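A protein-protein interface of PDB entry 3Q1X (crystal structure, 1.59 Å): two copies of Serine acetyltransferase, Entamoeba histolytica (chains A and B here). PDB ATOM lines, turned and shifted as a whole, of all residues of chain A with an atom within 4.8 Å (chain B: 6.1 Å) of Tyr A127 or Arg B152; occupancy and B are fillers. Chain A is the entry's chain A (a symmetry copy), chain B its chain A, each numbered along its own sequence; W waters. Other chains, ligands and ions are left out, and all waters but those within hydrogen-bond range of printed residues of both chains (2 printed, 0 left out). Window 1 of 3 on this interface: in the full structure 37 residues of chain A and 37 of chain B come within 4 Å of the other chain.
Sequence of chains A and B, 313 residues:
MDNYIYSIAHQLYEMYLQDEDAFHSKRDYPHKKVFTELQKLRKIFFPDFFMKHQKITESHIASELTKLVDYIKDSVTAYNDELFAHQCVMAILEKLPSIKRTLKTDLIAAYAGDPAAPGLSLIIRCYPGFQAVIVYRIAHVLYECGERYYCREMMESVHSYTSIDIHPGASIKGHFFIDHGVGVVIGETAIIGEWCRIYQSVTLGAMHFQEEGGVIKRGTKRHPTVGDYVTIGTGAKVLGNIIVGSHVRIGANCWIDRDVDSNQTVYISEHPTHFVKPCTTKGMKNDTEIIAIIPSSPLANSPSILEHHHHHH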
ATOM      1  N   ASP A 114     -14.040  12.904  -4.932  1.00  0.00           N
ATOM      2  CA  ASP A 114     -15.197  12.134  -5.404  1.00  0.00           C
ATOM      3  C   ASP A 114     -15.691  12.515  -6.813  1.00  0.00           C
ATOM      4  O   ASP A 114     -16.392  13.519  -6.985  1.00  0.00           O
ATOM      5  CB  ASP A 114     -16.362  12.247  -4.418  1.00  0.00           C
ATOM      6  CG  ASP A 114     -17.526  11.321  -4.778  1.00  0.00           C
ATOM      7  OD1 ASP A 114     -17.344  10.422  -5.634  1.00  0.00           O
ATOM      8  OD2 ASP A 114     -18.629  11.495  -4.210  1.00  0.00           O
ATOM      9  N   ALA A 116     -18.043  11.414  -8.358  1.00  0.00           N
ATOM     10  CA  ALA A 116     -19.505  11.366  -8.383  1.00  0.00           C
ATOM     11  C   ALA A 116     -20.175  12.663  -7.928  1.00  0.00           C
ATOM     12  O   ALA A 116     -21.364  12.838  -8.160  1.00  0.00           O
ATOM     13  CB  ALA A 116     -20.027  10.167  -7.561  1.00  0.00           C
ATOM     14  N   ALA A 117     -19.424  13.568  -7.290  1.00  0.00           N
ATOM     15  CA  ALA A 117     -20.010  14.798  -6.746  1.00  0.00           C
ATOM     16  C   ALA A 117     -20.161  15.876  -7.822  1.00  0.00           C
ATOM     17  O   ALA A 117     -19.177  16.256  -8.446  1.00  0.00           O
ATOM     18  CB  ALA A 117     -19.182  15.334  -5.559  1.00  0.00           C
ATOM     19  N   LEU A 122     -24.635  19.312  -3.139  1.00  0.00           N
ATOM     20  CA  LEU A 122     -25.117  17.938  -2.896  1.00  0.00           C
ATOM     21  C   LEU A 122     -24.416  17.276  -1.711  1.00  0.00           C
ATOM     22  O   LEU A 122     -25.018  16.475  -0.977  1.00  0.00           O
ATOM     23  CB  LEU A 122     -24.959  17.059  -4.142  1.00  0.00           C
ATOM     24  CG  LEU A 122     -25.751  15.748  -4.050  1.00  0.00           C
ATOM     25  CD1 LEU A 122     -27.260  16.036  -3.937  1.00  0.00           C
ATOM     26  CD2 LEU A 122     -25.456  14.870  -5.234  1.00  0.00           C
ATOM     27  N   ILE A 123     -23.140  17.614  -1.532  1.00  0.00           N
ATOM     28  CA  ILE A 123     -22.358  17.140  -0.399  1.00  0.00           C
ATOM     29  C   ILE A 123     -22.930  17.682   0.901  1.00  0.00           C
ATOM     30  O   ILE A 123     -23.163  16.929   1.856  1.00  0.00           O
ATOM     31  CB  ILE A 123     -20.860  17.512  -0.563  1.00  0.00           C
ATOM     32  CG1 ILE A 123     -20.354  17.035  -1.932  1.00  0.00           C
ATOM     33  CG2 ILE A 123     -20.034  16.904   0.570  1.00  0.00           C
ATOM     34  CD1 ILE A 123     -18.885  17.356  -2.224  1.00  0.00           C
ATOM     35  N   ARG A 125     -25.987  18.853   1.298  1.00  0.00           N
ATOM     36  CA  ARG A 125     -27.356  18.405   1.501  1.00  0.00           C
ATOM     37  C   ARG A 125     -27.463  16.978   2.019  1.00  0.00           C
ATOM     38  O   ARG A 125     -28.323  16.692   2.840  1.00  0.00           O
ATOM     39  CB  ARG A 125     -28.160  18.545   0.207  1.00  0.00           C
ATOM     40  CG  ARG A 125     -28.537  19.975  -0.140  1.00  0.00           C
ATOM     41  CD  ARG A 125     -29.716  20.452   0.681  1.00  0.00           C
ATOM     42  NE  ARG A 125     -30.884  19.605   0.471  1.00  0.00           N
ATOM     43  CZ  ARG A 125     -32.006  19.671   1.179  1.00  0.00           C
ATOM     44  NH1 ARG A 125     -32.121  20.539   2.185  1.00  0.00           N
ATOM     45  NH2 ARG A 125     -33.011  18.853   0.887  1.00  0.00           N
ATOM     46  N   CYS A 126     -26.603  16.073   1.550  1.00  0.00           N
ATOM     47  CA  CYS A 126     -26.881  14.652   1.793  1.00  0.00           C
ATOM     48  C   CYS A 126     -25.700  13.690   1.870  1.00  0.00           C
ATOM     49  O   CYS A 126     -25.923  12.500   2.025  1.00  0.00           O
ATOM     50  CB  CYS A 126     -27.864  14.128   0.741  1.00  0.00           C
ATOM     51  SG  CYS A 126     -27.092  13.802  -0.849  1.00  0.00           S
ATOM     52  N   TYR A 127     -24.461  14.168   1.764  1.00  0.00           N
ATOM     53  CA  TYR A 127     -23.322  13.233   1.868  1.00  0.00           C
ATOM     54  C   TYR A 127     -23.139  12.797   3.327  1.00  0.00           C
ATOM     55  O   TYR A 127     -22.942  13.642   4.197  1.00  0.00           O
ATOM     56  CB  TYR A 127     -22.033  13.841   1.319  1.00  0.00           C
ATOM     57  CG  TYR A 127     -21.770  13.555  -0.155  1.00  0.00           C
ATOM     58  CD1 TYR A 127     -20.509  13.125  -0.573  1.00  0.00           C
ATOM     59  CD2 TYR A 127     -22.774  13.695  -1.121  1.00  0.00           C
ATOM     60  CE1 TYR A 127     -20.248  12.855  -1.902  1.00  0.00           C
ATOM     61  CE2 TYR A 127     -22.519  13.431  -2.474  1.00  0.00           C
ATOM     62  CZ  TYR A 127     -21.253  12.997  -2.851  1.00  0.00           C
ATOM     63  OH  TYR A 127     -20.975  12.730  -4.178  1.00  0.00           O
ATOM     64  N   PRO A 128     -23.206  11.474   3.592  1.00  0.00           N
ATOM     65  CA  PRO A 128     -23.241  11.013   4.985  1.00  0.00           C
ATOM     66  C   PRO A 128     -21.933  11.248   5.758  1.00  0.00           C
ATOM     67  O   PRO A 128     -21.968  11.579   6.947  1.00  0.00           O
ATOM     68  CB  PRO A 128     -23.557   9.510   4.864  1.00  0.00           C
ATOM     69  CG  PRO A 128     -23.086   9.135   3.494  1.00  0.00           C
ATOM     70  CD  PRO A 128     -23.270  10.354   2.634  1.00  0.00           C
ATOM     71  N   GLY A 129     -20.792  11.061   5.089  1.00  0.00           N
ATOM     72  CA  GLY A 129     -19.495  11.423   5.674  1.00  0.00           C
ATOM     73  C   GLY A 129     -19.484  12.866   6.158  1.00  0.00           C
ATOM     74  O   GLY A 129     -18.934  13.160   7.221  1.00  0.00           O
ATOM     75  N   PHE A 130     -20.116  13.759   5.396  1.00  0.00           N
ATOM     76  CA  PHE A 130     -20.153  15.178   5.769  1.00  0.00           C
ATOM     77  C   PHE A 130     -21.120  15.477   6.923  1.00  0.00           C
ATOM     78  O   PHE A 130     -20.795  16.261   7.811  1.00  0.00           O
ATOM     79  CB  PHE A 130     -20.405  16.085   4.568  1.00  0.00           C
ATOM     80  CG  PHE A 130     -20.223  17.539   4.890  1.00  0.00           C
ATOM     81  CD1 PHE A 130     -18.958  18.040   5.194  1.00  0.00           C
ATOM     82  CD2 PHE A 130     -21.318  18.394   4.946  1.00  0.00           C
ATOM     83  CE1 PHE A 130     -18.784  19.380   5.528  1.00  0.00           C
ATOM     84  CE2 PHE A 130     -21.152  19.744   5.266  1.00  0.00           C
ATOM     85  CZ  PHE A 130     -19.890  20.233   5.565  1.00  0.00           C
ATOM     86  N   GLN A 131     -22.279  14.819   6.932  1.00  0.00           N
ATOM     87  CA  GLN A 131     -23.213  14.959   8.052  1.00  0.00           C
ATOM     88  C   GLN A 131     -22.552  14.533   9.360  1.00  0.00           C
ATOM     89  O   GLN A 131     -22.677  15.198  10.388  1.00  0.00           O
ATOM     90  CB  GLN A 131     -24.489  14.146   7.815  1.00  0.00           C
ATOM     91  CG  GLN A 131     -25.112  14.329   6.426  1.00  0.00           C
ATOM     92  CD  GLN A 131     -25.335  15.790   6.067  1.00  0.00           C
ATOM     93  OE1 GLN A 131     -25.923  16.544   6.848  1.00  0.00           O
ATOM     94  NE2 GLN A 131     -24.864  16.202   4.893  1.00  0.00           N
ATOM     95  N   PHE A 177     -12.286  13.652   4.526  1.00  0.00           N
ATOM     96  CA  PHE A 177     -13.349  13.056   3.709  1.00  0.00           C
ATOM     97  C   PHE A 177     -13.527  11.567   3.953  1.00  0.00           C
ATOM     98  O   PHE A 177     -12.594  10.781   3.773  1.00  0.00           O
ATOM     99  CB  PHE A 177     -13.091  13.324   2.223  1.00  0.00           C
ATOM    100  CG  PHE A 177     -14.139  12.750   1.288  1.00  0.00           C
ATOM    101  CD1 PHE A 177     -15.509  12.904   1.538  1.00  0.00           C
ATOM    102  CD2 PHE A 177     -13.747  12.104   0.118  1.00  0.00           C
ATOM    103  CE1 PHE A 177     -16.465  12.385   0.652  1.00  0.00           C
ATOM    104  CE2 PHE A 177     -14.691  11.588  -0.779  1.00  0.00           C
ATOM    105  CZ  PHE A 177     -16.052  11.726  -0.509  1.00  0.00           C
ATOM    106  N   ALA B 139     -35.101   5.747  -8.613  1.00  0.00           N
ATOM    107  CA  ALA B 139     -33.970   6.688  -8.644  1.00  0.00           C
ATOM    108  C   ALA B 139     -33.149   6.594  -9.939  1.00  0.00           C
ATOM    109  O   ALA B 139     -32.691   7.615 -10.479  1.00  0.00           O
ATOM    110  CB  ALA B 139     -33.081   6.493  -7.428  1.00  0.00           C
ATOM    111  N   GLU B 147     -30.785  13.724 -14.422  1.00  0.00           N
ATOM    112  CA  GLU B 147     -30.850  14.332 -13.100  1.00  0.00           C
ATOM    113  C   GLU B 147     -29.703  13.805 -12.232  1.00  0.00           C
ATOM    114  O   GLU B 147     -29.346  12.628 -12.316  1.00  0.00           O
ATOM    115  CB  GLU B 147     -32.223  14.081 -12.466  1.00  0.00           C
ATOM    116  CG  GLU B 147     -32.685  15.160 -11.489  1.00  0.00           C
ATOM    117  CD  GLU B 147     -32.072  15.017 -10.111  1.00  0.00           C
ATOM    118  OE1 GLU B 147     -31.889  13.863  -9.658  1.00  0.00           O
ATOM    119  OE2 GLU B 147     -31.775  16.053  -9.471  1.00  0.00           O
ATOM    120  N   ARG B 148     -29.114  14.679 -11.418  1.00  0.00           N
ATOM    121  CA  ARG B 148     -27.894  14.325 -10.706  1.00  0.00           C
ATOM    122  C   ARG B 148     -27.923  14.652  -9.212  1.00  0.00           C
ATOM    123  O   ARG B 148     -26.991  14.317  -8.489  1.00  0.00           O
ATOM    124  CB  ARG B 148     -26.686  14.999 -11.376  1.00  0.00           C
ATOM    125  CG  ARG B 148     -26.380  14.506 -12.803  1.00  0.00           C
ATOM    126  CD  ARG B 148     -25.804  13.098 -12.764  1.00  0.00           C
ATOM    127  NE  ARG B 148     -25.533  12.586 -14.103  1.00  0.00           N
ATOM    128  CZ  ARG B 148     -26.435  11.998 -14.886  1.00  0.00           C
ATOM    129  NH1 ARG B 148     -27.684  11.845 -14.472  1.00  0.00           N
ATOM    130  NH2 ARG B 148     -26.086  11.567 -16.093  1.00  0.00           N
ATOM    131  N   TYR B 149     -28.987  15.303  -8.758  1.00  0.00           N
ATOM    132  CA  TYR B 149     -29.066  15.763  -7.375  1.00  0.00           C
ATOM    133  C   TYR B 149     -30.097  15.014  -6.527  1.00  0.00           C
ATOM    134  O   TYR B 149     -29.740  14.314  -5.557  1.00  0.00           O
ATOM    135  CB  TYR B 149     -29.350  17.265  -7.349  1.00  0.00           C
ATOM    136  CG  TYR B 149     -28.131  18.106  -7.678  1.00  0.00           C
ATOM    137  CD1 TYR B 149     -27.734  18.293  -9.002  1.00  0.00           C
ATOM    138  CD2 TYR B 149     -27.375  18.707  -6.672  1.00  0.00           C
ATOM    139  CE1 TYR B 149     -26.613  19.049  -9.321  1.00  0.00           C
ATOM    140  CE2 TYR B 149     -26.242  19.477  -6.983  1.00  0.00           C
ATOM    141  CZ  TYR B 149     -25.874  19.636  -8.316  1.00  0.00           C
ATOM    142  OH  TYR B 149     -24.767  20.386  -8.657  1.00  0.00           O
ATOM    143  N   TYR B 150     -31.374  15.173  -6.868  1.00  0.00           N
ATOM    144  CA  TYR B 150     -32.424  14.562  -6.058  1.00  0.00           C
ATOM    145  C   TYR B 150     -32.360  13.025  -6.063  1.00  0.00           C
ATOM    146  O   TYR B 150     -32.595  12.398  -5.023  1.00  0.00           O
ATOM    147  CB  TYR B 150     -33.828  15.107  -6.404  1.00  0.00           C
ATOM    148  CG  TYR B 150     -34.936  14.292  -5.776  1.00  0.00           C
ATOM    149  CD1 TYR B 150     -35.090  14.220  -4.385  1.00  0.00           C
ATOM    150  CD2 TYR B 150     -35.809  13.568  -6.572  1.00  0.00           C
ATOM    151  CE1 TYR B 150     -36.100  13.434  -3.815  1.00  0.00           C
ATOM    152  CE2 TYR B 150     -36.817  12.803  -6.022  1.00  0.00           C
ATOM    153  CZ  TYR B 150     -36.961  12.732  -4.651  1.00  0.00           C
ATOM    154  OH  TYR B 150     -37.971  11.951  -4.131  1.00  0.00           O
ATOM    155  N   CYS B 151     -32.014  12.421  -7.208  1.00  0.00           N
ATOM    156  CA  CYS B 151     -31.873  10.949  -7.276  1.00  0.00           C
ATOM    157  C   CYS B 151     -30.798  10.438  -6.310  1.00  0.00           C
ATOM    158  O   CYS B 151     -30.944   9.361  -5.735  1.00  0.00           O
ATOM    159  CB  CYS B 151     -31.629  10.444  -8.714  1.00  0.00           C
ATOM    160  SG  CYS B 151     -30.067  10.987  -9.506  1.00  0.00           S
ATOM    161  N   ARG B 152     -29.741  11.226  -6.106  1.00  0.00           N
ATOM    162  CA  ARG B 152     -28.760  10.892  -5.078  1.00  0.00           C
ATOM    163  C   ARG B 152     -29.321  11.053  -3.661  1.00  0.00           C
ATOM    164  O   ARG B 152     -29.071  10.204  -2.802  1.00  0.00           O
ATOM    165  CB  ARG B 152     -27.467  11.697  -5.244  1.00  0.00           C
ATOM    166  CG  ARG B 152     -26.446  11.424  -4.136  1.00  0.00           C
ATOM    167  CD  ARG B 152     -25.882   9.995  -4.163  1.00  0.00           C
ATOM    168  NE  ARG B 152     -24.869   9.788  -3.120  1.00  0.00           N
ATOM    169  CZ  ARG B 152     -23.573  10.079  -3.239  1.00  0.00           C
ATOM    170  NH1 ARG B 152     -23.084  10.590  -4.367  1.00  0.00           N
ATOM    171  NH2 ARG B 152     -22.756   9.858  -2.220  1.00  0.00           N
ATOM    172  N   GLU B 153     -30.089  12.125  -3.423  1.00  0.00           N
ATOM    173  CA  GLU B 153     -30.702  12.368  -2.112  1.00  0.00           C
ATOM    174  C   GLU B 153     -31.644  11.229  -1.728  1.00  0.00           C
ATOM    175  O   GLU B 153     -31.634  10.749  -0.596  1.00  0.00           O
ATOM    176  CB  GLU B 153     -31.474  13.690  -2.102  1.00  0.00           C
ATOM    177  CG  GLU B 153     -32.017  14.081  -0.732  1.00  0.00           C
ATOM    178  CD  GLU B 153     -32.444  15.537  -0.675  1.00  0.00           C
ATOM    179  OE1 GLU B 153     -33.207  15.977  -1.562  1.00  0.00           O
ATOM    180  OE2 GLU B 153     -32.009  16.239   0.251  1.00  0.00           O
ATOM    181  N   MET B 154     -32.449  10.805  -2.697  1.00  0.00           N
ATOM    182  CA  MET B 154     -33.353   9.676  -2.508  1.00  0.00           C
ATOM    183  C   MET B 154     -32.592   8.426  -2.073  1.00  0.00           C
ATOM    184  O   MET B 154     -32.978   7.751  -1.114  1.00  0.00           O
ATOM    185  CB  MET B 154     -34.109   9.399  -3.805  1.00  0.00           C
ATOM    186  CG  MET B 154     -35.300   8.473  -3.645  1.00  0.00           C
ATOM    187  SD  MET B 154     -36.034   7.972  -5.222  1.00  0.00           S
ATOM    188  CE  MET B 154     -35.840   9.465  -6.145  1.00  0.00           C
ATOM    189  N   MET B 155     -31.491   8.129  -2.760  1.00  0.00           N
ATOM    190  CA  MET B 155     -30.691   6.955  -2.399  1.00  0.00           C
ATOM    191  C   MET B 155     -29.939   7.104  -1.068  1.00  0.00           C
ATOM    192  O   MET B 155     -29.637   6.102  -0.405  1.00  0.00           O
ATOM    193  CB  MET B 155     -29.725   6.577  -3.520  1.00  0.00           C
ATOM    194  CG  MET B 155     -30.398   6.108  -4.791  1.00  0.00           C
ATOM    195  SD  MET B 155     -31.727   4.936  -4.541  1.00  0.00           S
ATOM    196  CE  MET B 155     -30.819   3.500  -3.957  1.00  0.00           C
ATOM    197  N   GLU B 156     -29.667   8.339  -0.653  1.00  0.00           N
ATOM    198  CA  GLU B 156     -29.119   8.569   0.687  1.00  0.00           C
ATOM    199  C   GLU B 156     -30.140   8.287   1.807  1.00  0.00           C
ATOM    200  O   GLU B 156     -29.761   7.909   2.932  1.00  0.00           O
ATOM    201  CB  GLU B 156     -28.526   9.974   0.815  1.00  0.00           C
ATOM    202  CG  GLU B 156     -27.185  10.162   0.086  1.00  0.00           C
ATOM    203  CD  GLU B 156     -26.128   9.134   0.445  1.00  0.00           C
ATOM    204  OE1 GLU B 156     -26.102   8.639   1.592  1.00  0.00           O
ATOM    205  OE2 GLU B 156     -25.306   8.832  -0.439  1.00  0.00           O
ATOM    206  N   SER B 157     -31.428   8.448   1.502  1.00  0.00           N
ATOM    207  CA  SER B 157     -32.483   7.960   2.401  1.00  0.00           C
ATOM    208  C   SER B 157     -32.416   6.436   2.553  1.00  0.00           C
ATOM    209  O   SER B 157     -32.461   5.907   3.664  1.00  0.00           O
ATOM    210  CB  SER B 157     -33.871   8.390   1.932  1.00  0.00           C
ATOM    211  OG  SER B 157     -34.050   9.786   2.067  1.00  0.00           O
ATOM    212  N   ASP B 165     -25.697   1.151  -0.112  1.00  0.00           N
ATOM    213  CA  ASP B 165     -25.219   2.367  -0.754  1.00  0.00           C
ATOM    214  C   ASP B 165     -25.149   2.138  -2.252  1.00  0.00           C
ATOM    215  O   ASP B 165     -24.132   1.684  -2.767  1.00  0.00           O
ATOM    216  CB  ASP B 165     -23.827   2.723  -0.198  1.00  0.00           C
ATOM    217  CG  ASP B 165     -23.400   4.155  -0.521  1.00  0.00           C
ATOM    218  OD1 ASP B 165     -24.088   4.871  -1.302  1.00  0.00           O
ATOM    219  OD2 ASP B 165     -22.360   4.578   0.034  1.00  0.00           O
ATOM    220  N   ILE B 166     -26.234   2.449  -2.950  1.00  0.00           N
ATOM    221  CA  ILE B 166     -26.326   2.201  -4.381  1.00  0.00           C
ATOM    222  C   ILE B 166     -26.467   3.540  -5.070  1.00  0.00           C
ATOM    223  O   ILE B 166     -27.466   4.239  -4.867  1.00  0.00           O
ATOM    224  CB  ILE B 166     -27.555   1.319  -4.750  1.00  0.00           C
ATOM    225  CG1 ILE B 166     -27.505  -0.032  -4.036  1.00  0.00           C
ATOM    226  CG2 ILE B 166     -27.629   1.124  -6.271  1.00  0.00           C
ATOM    227  CD1 ILE B 166     -28.699  -0.936  -4.341  1.00  0.00           C
ATOM    228  N   HIS B 167     -25.470   3.920  -5.860  1.00  0.00           N
ATOM    229  CA  HIS B 167     -25.566   5.170  -6.604  1.00  0.00           C
ATOM    230  C   HIS B 167     -26.685   5.077  -7.642  1.00  0.00           C
ATOM    231  O   HIS B 167     -26.793   4.053  -8.323  1.00  0.00           O
ATOM    232  CB  HIS B 167     -24.251   5.529  -7.293  1.00  0.00           C
ATOM    233  CG  HIS B 167     -24.248   6.912  -7.853  1.00  0.00           C
ATOM    234  ND1 HIS B 167     -23.640   7.974  -7.218  1.00  0.00           N
ATOM    235  CD2 HIS B 167     -24.841   7.423  -8.958  1.00  0.00           C
ATOM    236  CE1 HIS B 167     -23.825   9.072  -7.930  1.00  0.00           C
ATOM    237  NE2 HIS B 167     -24.547   8.765  -8.991  1.00  0.00           N
ATOM    238  N   PRO B 168     -27.535   6.126  -7.752  1.00  0.00           N
ATOM    239  CA  PRO B 168     -28.635   6.057  -8.718  1.00  0.00           C
ATOM    240  C   PRO B 168     -28.211   5.793 -10.162  1.00  0.00           C
ATOM    241  O   PRO B 168     -29.038   5.359 -10.961  1.00  0.00           O
ATOM    242  CB  PRO B 168     -29.308   7.437  -8.590  1.00  0.00           C
ATOM    243  CG  PRO B 168     -28.282   8.318  -7.922  1.00  0.00           C
ATOM    244  CD  PRO B 168     -27.599   7.376  -6.969  1.00  0.00           C
HETATM  245  O   HOH W   1     -23.673  11.752  -6.932  1.00  0.00           O
HETATM  246  O   HOH W   2     -19.758   9.318  -3.144  1.00  0.00           O
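Of the 13 printed residues of chain A, 6 touch a printed residue of chain B. Printed residues of chain A that touch a printed residue of chain B: Ala A116, Leu A122, Arg A125, Cys A126, Tyr A127 and Pro A128. Hydrophobic or aromatic side chains of chain A that line the printed part of chain B: Ala A116, Leu A122, Tyr A127 and Pro A128. Of the 16 printed residues of chain B, 6 touch a printed residue of chain A. Printed residues of chain B that touch a printed residue of chain A: Arg B148, Tyr B149, Arg B152, Glu B153, Glu B156 and His B167. Among the printed residues, Asp or Glu carboxylates within 4 Å of a Lys or Arg side-chain nitrogen of the other chain: Arg A125 with Glu B153 (2.9 Å).
The side-chain carboxylate (OE2) of Glu B147 lies within hydrogen-bond range of the backbone NH (N) of Tyr B149 (3.0 Å). The side-chain carboxylate (OE2) of Glu B156 lies within salt-bridge range of the guanidinium group (NE) of Arg B152, 2.9 Å away. The side-chain carboxylate of Asp A114 sits at hydrogen-bond distance from the backbone NH of Ala A116 (3.0 Å). The side-chain hydroxyl of Tyr A127 is in hydrogen-bond range of the side-chain carboxylate of Asp A114, 2.7 Å away. The backbone carbonyl oxygen (O) of Leu A122 lies within hydrogen-bond range of the side-chain sulfur (SG) of Cys A126 (3.4 Å). The backbone carbonyl oxygen (O) of Tyr A127 sits close to the side-chain amide nitrogen (NE2) of Gln A131, at 3.3 Å.
Water W2 bridges the side-chain carboxylate of Asp A114 and the guanidinium group of Arg B152. Water W1 bridges O of Ala A116 (2.8 Å) and NH1 of Arg B152 (2.9 Å).
No position is printed for both chains. Of the 8 pairs that touch across the chains among the printed residues, none has its exchanged pair printed and touching as well.
Tyr A127 touches just one residue of chain B: Arg B152. Arg B152 touches just these residues of chain A: Leu A122 and Tyr A127. Printed residues of chain B within 4 Å of Cys A126: Glu B156. Of the printed residues of chain A, Tyr B149 touches Leu A122 (3.4 Å). Printed residues of chain A within 4 Å of Glu B153: Arg A125. Asp A114 touches none of the printed residues of chain B. The nearest residue of chain B that does not touch Tyr A127 is Glu B156 (5.1 Å). The nearest residue of chain A that does not touch Arg B152 is Cys A126 (4.1 Å). The nearest printed residue of chain B that does not touch Cys A126 is Glu B153 (4.1 Å).
The guanidinium group (NH1) of Arg B152 is in hydrogen-bond range of the side-chain hydroxyl (OH) of Tyr A127, at 3.0 Å. The guanidinium group (NH2) of Arg A125 is in salt-bridge range of the side-chain carboxylate (OE2) of Glu B153, at 2.9 Å.
Among the printed residues, pairs that only touch across the chains: Cys A126 with Glu B156 (3.3 Å), Leu A122 with Tyr B149 (3.4 Å), Pro A128 with Glu B156 (3.5 Å), Leu A122 with Arg B148 (3.6 Å), Leu A122 with Arg B152 (3.7 Å) and Ala A116 with His B167 (3.97 Å).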
